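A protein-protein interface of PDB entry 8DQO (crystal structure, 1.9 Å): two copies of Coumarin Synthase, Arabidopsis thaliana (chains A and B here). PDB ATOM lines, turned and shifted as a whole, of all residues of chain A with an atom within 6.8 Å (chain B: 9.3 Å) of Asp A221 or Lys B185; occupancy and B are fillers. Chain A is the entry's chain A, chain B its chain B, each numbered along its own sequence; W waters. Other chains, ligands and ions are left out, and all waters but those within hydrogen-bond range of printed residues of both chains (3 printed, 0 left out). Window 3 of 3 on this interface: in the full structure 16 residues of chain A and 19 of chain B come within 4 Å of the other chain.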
ATOM      1  N   ASN A  34      -0.792 -17.594  11.769  1.00  0.00           N
ATOM      2  CA  ASN A  34       0.092 -16.686  12.535  1.00  0.00           C
ATOM      3  C   ASN A  34      -0.556 -16.217  13.855  1.00  0.00           C
ATOM      4  O   ASN A  34       0.146 -15.965  14.812  1.00  0.00           O
ATOM      5  CB  ASN A  34       0.539 -15.475  11.711  1.00  0.00           C
ATOM      6  CG  ASN A  34       1.559 -14.633  12.439  1.00  0.00           C
ATOM      7  OD1 ASN A  34       1.326 -13.441  12.684  1.00  0.00           O
ATOM      8  ND2 ASN A  34       2.677 -15.236  12.793  1.00  0.00           N
ATOM      9  N   ARG A  82      10.754 -24.043  12.031  1.00  0.00           N
ATOM     10  CA  ARG A  82      10.344 -23.653  10.691  1.00  0.00           C
ATOM     11  C   ARG A  82      10.860 -24.710   9.712  1.00  0.00           C
ATOM     12  O   ARG A  82      11.947 -25.226   9.866  1.00  0.00           O
ATOM     13  CB  ARG A  82      10.804 -22.226  10.400  1.00  0.00           C
ATOM     14  CG  ARG A  82      10.096 -21.200  11.277  1.00  0.00           C
ATOM     15  CD  ARG A  82      10.724 -19.825  11.276  1.00  0.00           C
ATOM     16  NE  ARG A  82       9.877 -18.870  11.972  1.00  0.00           N
ATOM     17  CZ  ARG A  82      10.002 -18.546  13.264  1.00  0.00           C
ATOM     18  NH1 ARG A  82      10.984 -19.060  13.984  1.00  0.00           N
ATOM     19  NH2 ARG A  82       9.107 -17.748  13.827  1.00  0.00           N
ATOM     20  N   ARG A 133       6.622 -16.133  22.260  1.00  0.00           N
ATOM     21  CA  ARG A 133       6.166 -16.990  21.143  1.00  0.00           C
ATOM     22  C   ARG A 133       7.350 -17.815  20.595  1.00  0.00           C
ATOM     23  O   ARG A 133       7.206 -19.006  20.335  1.00  0.00           O
ATOM     24  CB  ARG A 133       5.483 -16.141  20.063  1.00  0.00           C
ATOM     25  CG  ARG A 133       6.330 -15.009  19.491  1.00  0.00           C
ATOM     26  CD  ARG A 133       5.753 -14.352  18.237  1.00  0.00           C
ATOM     27  NE  ARG A 133       6.128 -12.953  18.031  1.00  0.00           N
ATOM     28  CZ  ARG A 133       7.368 -12.458  17.787  1.00  0.00           C
ATOM     29  NH1 ARG A 133       8.422 -13.225  17.573  1.00  0.00           N
ATOM     30  NH2 ARG A 133       7.535 -11.154  17.697  1.00  0.00           N
ATOM     31  N   GLU A 134       8.538 -17.198  20.480  1.00  0.00           N
ATOM     32  CA  GLU A 134       9.733 -17.884  19.936  1.00  0.00           C
ATOM     33  C   GLU A 134      10.290 -18.884  20.961  1.00  0.00           C
ATOM     34  O   GLU A 134      10.675 -20.005  20.616  1.00  0.00           O
ATOM     35  CB  GLU A 134      10.748 -16.855  19.447  1.00  0.00           C
ATOM     36  CG  GLU A 134      10.213 -15.931  18.360  1.00  0.00           C
ATOM     37  CD  GLU A 134       9.879 -16.617  17.038  1.00  0.00           C
ATOM     38  OE1 GLU A 134      10.580 -17.573  16.665  1.00  0.00           O
ATOM     39  OE2 GLU A 134       8.920 -16.172  16.377  1.00  0.00           O
ATOM     40  N   ASP A 217      -1.165  -7.860   5.044  1.00  0.00           N
ATOM     41  CA  ASP A 217      -0.235  -6.764   5.341  1.00  0.00           C
ATOM     42  C   ASP A 217       0.992  -7.375   6.020  1.00  0.00           C
ATOM     43  O   ASP A 217       0.939  -7.736   7.177  1.00  0.00           O
ATOM     44  CB  ASP A 217      -0.935  -5.695   6.186  1.00  0.00           C
ATOM     45  CG  ASP A 217      -0.130  -4.421   6.415  1.00  0.00           C
ATOM     46  OD1 ASP A 217       1.077  -4.421   6.122  1.00  0.00           O
ATOM     47  OD2 ASP A 217      -0.747  -3.435   6.857  1.00  0.00           O
ATOM     48  N   LYS A 218       2.077  -7.517   5.278  1.00  0.00           N
ATOM     49  CA  LYS A 218       3.315  -8.066   5.850  1.00  0.00           C
ATOM     50  C   LYS A 218       3.851  -7.168   6.984  1.00  0.00           C
ATOM     51  O   LYS A 218       4.694  -7.621   7.751  1.00  0.00           O
ATOM     52  CB  LYS A 218       4.400  -8.215   4.790  1.00  0.00           C
ATOM     53  CG  LYS A 218       4.189  -9.316   3.761  1.00  0.00           C
ATOM     54  CD  LYS A 218       5.294  -9.333   2.717  1.00  0.00           C
ATOM     55  CE  LYS A 218       4.806  -8.911   1.346  1.00  0.00           C
ATOM     56  NZ  LYS A 218       4.202 -10.071   0.643  1.00  0.00           N
ATOM     57  N   ASP A 219       3.392  -5.922   7.074  1.00  0.00           N
ATOM     58  CA  ASP A 219       3.953  -4.924   8.014  1.00  0.00           C
ATOM     59  C   ASP A 219       3.098  -4.831   9.290  1.00  0.00           C
ATOM     60  O   ASP A 219       3.376  -3.968  10.141  1.00  0.00           O
ATOM     61  CB  ASP A 219       4.057  -3.551   7.358  1.00  0.00           C
ATOM     62  CG  ASP A 219       4.944  -3.542   6.120  1.00  0.00           C
ATOM     63  OD1 ASP A 219       5.933  -4.257   6.115  1.00  0.00           O
ATOM     64  OD2 ASP A 219       4.605  -2.830   5.160  1.00  0.00           O
ATOM     65  N   PHE A 220       2.082  -5.696   9.427  1.00  0.00           N
ATOM     66  CA  PHE A 220       1.160  -5.592  10.542  1.00  0.00           C
ATOM     67  C   PHE A 220       1.363  -6.778  11.480  1.00  0.00           C
ATOM     68  O   PHE A 220       1.293  -7.915  11.042  1.00  0.00           O
ATOM     69  CB  PHE A 220      -0.299  -5.542  10.070  1.00  0.00           C
ATOM     70  CG  PHE A 220      -1.332  -5.464  11.170  1.00  0.00           C
ATOM     71  CD1 PHE A 220      -1.455  -4.316  11.943  1.00  0.00           C
ATOM     72  CD2 PHE A 220      -2.138  -6.549  11.473  1.00  0.00           C
ATOM     73  CE1 PHE A 220      -2.393  -4.252  12.961  1.00  0.00           C
ATOM     74  CE2 PHE A 220      -3.082  -6.486  12.500  1.00  0.00           C
ATOM     75  CZ  PHE A 220      -3.229  -5.319  13.213  1.00  0.00           C
ATOM     76  N   ASP A 221       1.565  -6.482  12.772  1.00  0.00           N
ATOM     77  CA  ASP A 221       1.637  -7.521  13.826  1.00  0.00           C
ATOM     78  C   ASP A 221       0.411  -7.342  14.705  1.00  0.00           C
ATOM     79  O   ASP A 221       0.333  -6.372  15.452  1.00  0.00           O
ATOM     80  CB  ASP A 221       2.944  -7.405  14.630  1.00  0.00           C
ATOM     81  CG  ASP A 221       3.138  -8.446  15.731  1.00  0.00           C
ATOM     82  OD1 ASP A 221       2.260  -9.289  15.946  1.00  0.00           O
ATOM     83  OD2 ASP A 221       4.186  -8.410  16.379  1.00  0.00           O
ATOM     84  N   PRO A 222      -0.591  -8.247  14.646  1.00  0.00           N
ATOM     85  CA  PRO A 222      -1.797  -8.099  15.451  1.00  0.00           C
ATOM     86  C   PRO A 222      -1.506  -8.024  16.958  1.00  0.00           C
ATOM     87  O   PRO A 222      -2.303  -7.458  17.667  1.00  0.00           O
ATOM     88  CB  PRO A 222      -2.591  -9.384  15.217  1.00  0.00           C
ATOM     89  CG  PRO A 222      -1.561 -10.345  14.702  1.00  0.00           C
ATOM     90  CD  PRO A 222      -0.583  -9.517  13.905  1.00  0.00           C
ATOM     91  N   TYR A 223      -0.409  -8.646  17.401  1.00  0.00           N
ATOM     92  CA  TYR A 223      -0.082  -8.669  18.810  1.00  0.00           C
ATOM     93  C   TYR A 223       1.005  -7.654  19.168  1.00  0.00           C
ATOM     94  O   TYR A 223       1.514  -7.696  20.292  1.00  0.00           O
ATOM     95  CB  TYR A 223       0.339 -10.079  19.222  1.00  0.00           C
ATOM     96  CG  TYR A 223      -0.715 -11.126  18.965  1.00  0.00           C
ATOM     97  CD1 TYR A 223      -2.053 -10.895  19.263  1.00  0.00           C
ATOM     98  CD2 TYR A 223      -0.379 -12.366  18.451  1.00  0.00           C
ATOM     99  CE1 TYR A 223      -3.026 -11.853  19.042  1.00  0.00           C
ATOM    100  CE2 TYR A 223      -1.341 -13.329  18.214  1.00  0.00           C
ATOM    101  CZ  TYR A 223      -2.666 -13.082  18.529  1.00  0.00           C
ATOM    102  OH  TYR A 223      -3.646 -14.007  18.299  1.00  0.00           O
ATOM    103  N   GLY A 224       1.331  -6.739  18.255  1.00  0.00           N
ATOM    104  CA  GLY A 224       2.370  -5.734  18.504  1.00  0.00           C
ATOM    105  C   GLY A 224       1.866  -4.323  18.331  1.00  0.00           C
ATOM    106  O   GLY A 224       2.661  -3.455  18.057  1.00  0.00           O
ATOM    107  N   GLN A 225       0.553  -4.120  18.461  1.00  0.00           N
ATOM    108  CA  GLN A 225      -0.046  -2.841  18.253  1.00  0.00           C
ATOM    109  C   GLN A 225       0.276  -1.946  19.464  1.00  0.00           C
ATOM    110  O   GLN A 225       0.431  -2.433  20.584  1.00  0.00           O
ATOM    111  CB  GLN A 225      -1.546  -2.971  18.015  1.00  0.00           C
ATOM    112  CG  GLN A 225      -1.914  -3.861  16.836  1.00  0.00           C
ATOM    113  CD  GLN A 225      -3.404  -4.069  16.756  1.00  0.00           C
ATOM    114  OE1 GLN A 225      -3.910  -5.188  16.950  1.00  0.00           O
ATOM    115  NE2 GLN A 225      -4.120  -2.990  16.494  1.00  0.00           N
ATOM    116  N   MET A 400      -5.432  -8.189  21.042  1.00  0.00           N
ATOM    117  CA  MET A 400      -4.597  -7.936  22.225  1.00  0.00           C
ATOM    118  C   MET A 400      -5.467  -7.687  23.469  1.00  0.00           C
ATOM    119  O   MET A 400      -4.944  -7.410  24.549  1.00  0.00           O
ATOM    120  CB  MET A 400      -3.704  -6.717  21.989  1.00  0.00           C
ATOM    121  CG  MET A 400      -2.571  -7.013  21.049  1.00  0.00           C
ATOM    122  SD  MET A 400      -1.685  -5.537  20.609  1.00  0.00           S
ATOM    123  CE  MET A 400      -0.703  -5.321  22.102  1.00  0.00           C
ATOM    124  N   THR B  68      22.308  -9.530  12.848  1.00  0.00           N
ATOM    125  CA  THR B  68      20.901  -9.094  12.800  1.00  0.00           C
ATOM    126  C   THR B  68      20.463  -8.550  14.171  1.00  0.00           C
ATOM    127  O   THR B  68      19.702  -7.575  14.216  1.00  0.00           O
ATOM    128  CB  THR B  68      19.964 -10.211  12.305  1.00  0.00           C
ATOM    129  OG1 THR B  68      20.416 -10.708  11.048  1.00  0.00           O
ATOM    130  CG2 THR B  68      18.531  -9.745  12.141  1.00  0.00           C
ATOM    131  N   HIS B  72      19.231  -3.953  16.644  1.00  0.00           N
ATOM    132  CA  HIS B  72      18.474  -3.494  17.794  1.00  0.00           C
ATOM    133  C   HIS B  72      19.388  -3.287  19.020  1.00  0.00           C
ATOM    134  O   HIS B  72      19.159  -2.370  19.814  1.00  0.00           O
ATOM    135  CB  HIS B  72      17.362  -4.505  18.100  1.00  0.00           C
ATOM    136  CG  HIS B  72      16.431  -4.747  16.954  1.00  0.00           C
ATOM    137  ND1 HIS B  72      15.365  -3.917  16.701  1.00  0.00           N
ATOM    138  CD2 HIS B  72      16.407  -5.705  16.002  1.00  0.00           C
ATOM    139  CE1 HIS B  72      14.717  -4.341  15.634  1.00  0.00           C
ATOM    140  NE2 HIS B  72      15.338  -5.451  15.186  1.00  0.00           N
ATOM    141  N   ASN B 174      18.699 -14.404  23.641  1.00  0.00           N
ATOM    142  CA  ASN B 174      17.474 -14.986  23.179  1.00  0.00           C
ATOM    143  C   ASN B 174      17.084 -14.359  21.842  1.00  0.00           C
ATOM    144  O   ASN B 174      16.514 -15.050  20.982  1.00  0.00           O
ATOM    145  CB  ASN B 174      16.355 -14.852  24.209  1.00  0.00           C
ATOM    146  CG  ASN B 174      16.246 -16.074  25.083  1.00  0.00           C
ATOM    147  OD1 ASN B 174      15.834 -17.133  24.607  1.00  0.00           O
ATOM    148  ND2 ASN B 174      16.586 -15.932  26.349  1.00  0.00           N
ATOM    149  N   ALA B 175      17.412 -13.074  21.654  1.00  0.00           N
ATOM    150  CA  ALA B 175      17.167 -12.398  20.362  1.00  0.00           C
ATOM    151  C   ALA B 175      18.025 -13.058  19.274  1.00  0.00           C
ATOM    152  O   ALA B 175      17.534 -13.383  18.199  1.00  0.00           O
ATOM    153  CB  ALA B 175      17.443 -10.918  20.488  1.00  0.00           C
ATOM    154  N   MET B 176      19.313 -13.281  19.567  1.00  0.00           N
ATOM    155  CA  MET B 176      20.182 -13.953  18.612  1.00  0.00           C
ATOM    156  C   MET B 176      19.626 -15.351  18.294  1.00  0.00           C
ATOM    157  O   MET B 176      19.545 -15.733  17.127  1.00  0.00           O
ATOM    158  CB  MET B 176      21.607 -14.092  19.153  1.00  0.00           C
ATOM    159  CG  MET B 176      22.393 -12.789  19.138  1.00  0.00           C
ATOM    160  SD  MET B 176      24.061 -13.003  19.849  1.00  0.00           S
ATOM    161  CE  MET B 176      24.730 -14.254  18.759  1.00  0.00           C
ATOM    162  N   ALA B 177      19.279 -16.114  19.346  1.00  0.00           N
ATOM    163  CA  ALA B 177      18.856 -17.510  19.169  1.00  0.00           C
ATOM    164  C   ALA B 177      17.576 -17.581  18.329  1.00  0.00           C
ATOM    165  O   ALA B 177      17.450 -18.474  17.478  1.00  0.00           O
ATOM    166  CB  ALA B 177      18.656 -18.191  20.503  1.00  0.00           C
ATOM    167  N   GLU B 178      16.609 -16.688  18.594  1.00  0.00           N
ATOM    168  CA  GLU B 178      15.294 -16.766  17.881  1.00  0.00           C
ATOM    169  C   GLU B 178      15.497 -16.374  16.412  1.00  0.00           C
ATOM    170  O   GLU B 178      14.887 -16.978  15.517  1.00  0.00           O
ATOM    171  CB  GLU B 178      14.181 -15.927  18.525  1.00  0.00           C
ATOM    172  CG  GLU B 178      14.380 -14.407  18.464  1.00  0.00           C
ATOM    173  CD  GLU B 178      13.299 -13.589  19.202  1.00  0.00           C
ATOM    174  OE1 GLU B 178      13.530 -12.377  19.411  1.00  0.00           O
ATOM    175  OE2 GLU B 178      12.342 -14.186  19.698  1.00  0.00           O
ATOM    176  N   LEU B 179      16.377 -15.394  16.159  1.00  0.00           N
ATOM    177  CA  LEU B 179      16.729 -15.042  14.765  1.00  0.00           C
ATOM    178  C   LEU B 179      17.452 -16.218  14.103  1.00  0.00           C
ATOM    179  O   LEU B 179      17.192 -16.534  12.952  1.00  0.00           O
ATOM    180  CB  LEU B 179      17.596 -13.782  14.756  1.00  0.00           C
ATOM    181  CG  LEU B 179      16.890 -12.511  15.208  1.00  0.00           C
ATOM    182  CD1 LEU B 179      17.915 -11.419  15.507  1.00  0.00           C
ATOM    183  CD2 LEU B 179      15.887 -12.029  14.176  1.00  0.00           C
ATOM    184  N   ALA B 180      18.313 -16.915  14.848  1.00  0.00           N
ATOM    185  CA  ALA B 180      19.007 -18.091  14.294  1.00  0.00           C
ATOM    186  C   ALA B 180      17.981 -19.174  13.908  1.00  0.00           C
ATOM    187  O   ALA B 180      18.195 -19.924  12.969  1.00  0.00           O
ATOM    188  CB  ALA B 180      20.020 -18.601  15.279  1.00  0.00           C
ATOM    189  N   ARG B 181      16.838 -19.198  14.609  1.00  0.00           N
ATOM    190  CA  ARG B 181      15.754 -20.199  14.426  1.00  0.00           C
ATOM    191  C   ARG B 181      14.753 -19.712  13.367  1.00  0.00           C
ATOM    192  O   ARG B 181      13.768 -20.416  13.035  1.00  0.00           O
ATOM    193  CB  ARG B 181      15.084 -20.508  15.774  1.00  0.00           C
ATOM    194  CG  ARG B 181      15.938 -21.326  16.737  1.00  0.00           C
ATOM    195  CD  ARG B 181      15.189 -21.807  17.979  1.00  0.00           C
ATOM    196  NE  ARG B 181      14.370 -20.806  18.669  1.00  0.00           N
ATOM    197  CZ  ARG B 181      14.713 -20.111  19.738  1.00  0.00           C
ATOM    198  NH1 ARG B 181      15.940 -20.193  20.251  1.00  0.00           N
ATOM    199  NH2 ARG B 181      13.804 -19.329  20.307  1.00  0.00           N
ATOM    200  N   GLY B 182      15.027 -18.539  12.781  1.00  0.00           N
ATOM    201  CA  GLY B 182      14.311 -18.056  11.603  1.00  0.00           C
ATOM    202  C   GLY B 182      13.154 -17.134  11.947  1.00  0.00           C
ATOM    203  O   GLY B 182      12.248 -16.936  11.115  1.00  0.00           O
ATOM    204  N   ALA B 183      13.145 -16.593  13.163  1.00  0.00           N
ATOM    205  CA  ALA B 183      12.194 -15.566  13.496  1.00  0.00           C
ATOM    206  C   ALA B 183      12.235 -14.492  12.376  1.00  0.00           C
ATOM    207  O   ALA B 183      13.348 -14.172  11.761  1.00  0.00           O
ATOM    208  CB  ALA B 183      12.451 -15.018  14.873  1.00  0.00           C
ATOM    209  N   THR B 184      11.022 -13.929  12.141  1.00  0.00           N
ATOM    210  CA  THR B 184      10.911 -12.854  11.172  1.00  0.00           C
ATOM    211  C   THR B 184      11.162 -11.516  11.885  1.00  0.00           C
ATOM    212  O   THR B 184      11.448 -10.509  11.246  1.00  0.00           O
ATOM    213  CB  THR B 184       9.572 -12.954  10.438  1.00  0.00           C
ATOM    214  OG1 THR B 184       9.634 -11.916   9.467  1.00  0.00           O
ATOM    215  CG2 THR B 184       8.361 -12.789  11.329  1.00  0.00           C
ATOM    216  N   LYS B 185      11.041 -11.515  13.215  1.00  0.00           N
ATOM    217  CA  LYS B 185      11.437 -10.373  14.045  1.00  0.00           C
ATOM    218  C   LYS B 185      11.560 -10.814  15.507  1.00  0.00           C
ATOM    219  O   LYS B 185      10.913 -11.780  15.925  1.00  0.00           O
ATOM    220  CB  LYS B 185      10.433  -9.222  13.928  1.00  0.00           C
ATOM    221  CG  LYS B 185       9.096  -9.413  14.636  1.00  0.00           C
ATOM    222  CD  LYS B 185       8.434  -8.080  14.920  1.00  0.00           C
ATOM    223  CE  LYS B 185       6.946  -8.173  15.147  1.00  0.00           C
ATOM    224  NZ  LYS B 185       6.322  -6.831  15.096  1.00  0.00           N
ATOM    225  N   ILE B 186      12.304 -10.024  16.286  1.00  0.00           N
ATOM    226  CA  ILE B 186      12.610 -10.349  17.660  1.00  0.00           C
ATOM    227  C   ILE B 186      11.330 -10.222  18.507  1.00  0.00           C
ATOM    228  O   ILE B 186      10.472  -9.423  18.206  1.00  0.00           O
ATOM    229  CB  ILE B 186      13.777  -9.473  18.154  1.00  0.00           C
ATOM    230  CG1 ILE B 186      13.437  -7.978  18.174  1.00  0.00           C
ATOM    231  CG2 ILE B 186      15.016  -9.741  17.312  1.00  0.00           C
ATOM    232  CD1 ILE B 186      14.524  -7.128  18.787  1.00  0.00           C
ATOM    233  N   SER B 187      11.208 -11.042  19.557  1.00  0.00           N
ATOM    234  CA  SER B 187       9.982 -11.142  20.385  1.00  0.00           C
ATOM    235  C   SER B 187       9.772  -9.886  21.252  1.00  0.00           C
ATOM    236  O   SER B 187       8.635  -9.508  21.524  1.00  0.00           O
ATOM    237  CB  SER B 187      10.024 -12.385  21.245  1.00  0.00           C
ATOM    238  OG  SER B 187       9.882 -13.544  20.438  1.00  0.00           O
ATOM    239  N   ILE B 188      10.869  -9.279  21.723  1.00  0.00           N
ATOM    240  CA  ILE B 188      10.816  -8.122  22.636  1.00  0.00           C
ATOM    241  C   ILE B 188      11.823  -7.083  22.145  1.00  0.00           C
ATOM    242  O   ILE B 188      13.020  -7.348  22.162  1.00  0.00           O
ATOM    243  CB  ILE B 188      11.125  -8.536  24.086  1.00  0.00           C
ATOM    244  CG1 ILE B 188      10.205  -9.660  24.576  1.00  0.00           C
ATOM    245  CG2 ILE B 188      11.089  -7.331  25.031  1.00  0.00           C
ATOM    246  CD1 ILE B 188      10.588 -10.195  25.948  1.00  0.00           C
ATOM    247  N   GLU B 189      11.325  -5.914  21.729  1.00  0.00           N
ATOM    248  CA  GLU B 189      12.193  -4.820  21.310  1.00  0.00           C
ATOM    249  C   GLU B 189      12.882  -4.237  22.546  1.00  0.00           C
ATOM    250  O   GLU B 189      12.216  -3.911  23.528  1.00  0.00           O
ATOM    251  CB  GLU B 189      11.415  -3.729  20.578  1.00  0.00           C
ATOM    252  CG  GLU B 189      12.249  -3.042  19.506  1.00  0.00           C
ATOM    253  CD  GLU B 189      11.535  -1.927  18.764  1.00  0.00           C
ATOM    254  OE1 GLU B 189      11.846  -0.740  19.057  1.00  0.00           O
ATOM    255  OE2 GLU B 189      10.672  -2.232  17.894  1.00  0.00           O
HETATM  256  O   HOH W   1      12.040 -19.947  17.384  1.00  0.00           O
HETATM  257  O   HOH W   2       8.792 -14.489  14.172  1.00  0.00           O
HETATM  258  O   HOH W   3      12.871 -22.766  13.425  1.00  0.00           O
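Printed residues of chain A that touch a printed residue of chain B: Arg A82, Arg A133, Glu A134 and Asp A221. Of the 18 printed residues of chain B, 7 touch a printed residue of chain A. Hydrophobic or aromatic side chains of chain B that line the printed part of chain A: Ala B183. Along chain B the printed residues that touch a printed residue of chain A span positions 178 to 187. Among the printed residues, Asp or Glu carboxylates within 4 Å of a Lys or Arg side-chain nitrogen of the other chain: Asp A221 with Lys B185 (2.9 Å).
Of chain B, only Lys B185 comes within 4 Å of Asp A221. No residue of chain B comes within 4 Å of Phe A220. No residue of chain B comes within 4 Å of Pro A222. No residue of chain B comes within 4 Å of Gly A224. Of the printed residues of chain A, Ser B187 touches Arg A133 and Glu A134. Of the printed residues of chain A, Ala B183 touches Arg A82 and Glu A134. Printed residues of chain A within 4 Å of Arg B181: Arg A82 and Glu A134. Printed residues of chain B within 4 Å of Glu A134: Glu B178, Arg B181, Ala B183 and Ser B187. The nearest residue of chain B that does not touch Asp A221 is Ile B186 (6.6 Å). The nearest residue of chain A that does not touch Lys B185 is Glu A134 (4.8 Å). The nearest printed residue of chain A that does not touch Arg B181 is Arg A133 (6.6 Å).
CG of Glu A134 touches OE2 of Glu B178, at 3.1 Å. OE1 of Glu A134 touches CB of Ala B183, 3.6 Å away. Ser B187 touches Glu A134 (OG to CG, 3.2 Å).
No position is printed for both chains.
NH1 of Arg A82 is in hydrogen-bond range of O of Arg B181 (3.2 Å). The guanidinium group (NE) of Arg A82 lies within hydrogen-bond range of the backbone carbonyl oxygen (O) of Gly B182, 3.2 Å away. O of Lys B185 sits at hydrogen-bond distance from NH1 of Arg A133 (3.3 Å). The backbone carbonyl oxygen of Ile B186 is in hydrogen-bond range of the guanidinium group of Arg A133, 3.4 Å away. NH1 of Arg A133 sits at hydrogen-bond distance from OG of Ser B187, at 3.2 Å. The guanidinium group (NH2) of Arg B181 lies within hydrogen-bond range of the backbone carbonyl oxygen (O) of Glu A134 (3.2 Å). OD2 of Asp A221 lies within salt-bridge range of NZ of Lys B185, 2.9 Å away. The backbone NH of Ala B183 sits close to the guanidinium group of Arg A82.
Water W3 bridges the backbone carbonyl oxygen of Arg B181 (2.5 Å) and the backbone NH of Arg A82 (2.8 Å). Water W2 lies within hydrogen-bond range of OE2 of Glu A134, N of Thr B184 and NH2 of Arg A82. Water W1 bridges NE of Arg B181 (2.8 Å) and OE1 of Glu A134 (2.9 Å).
The side-chain carboxylate (OE2) of Glu A134 is in salt-bridge range of the guanidinium group (NH2) of Arg A82. The side-chain carboxylate of Glu A134 lies within salt-bridge range of the guanidinium group of Arg A133 (3.2 Å). The backbone NH (N) of Tyr A223 lies close to the side-chain carboxylate (OD1) of Asp A221 (3.1 Å). The backbone NH of Ala B183 is in hydrogen-bond range of the backbone carbonyl oxygen of Glu B178. OG of Ser B187 sits at hydrogen-bond distance from OE2 of Glu B178.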
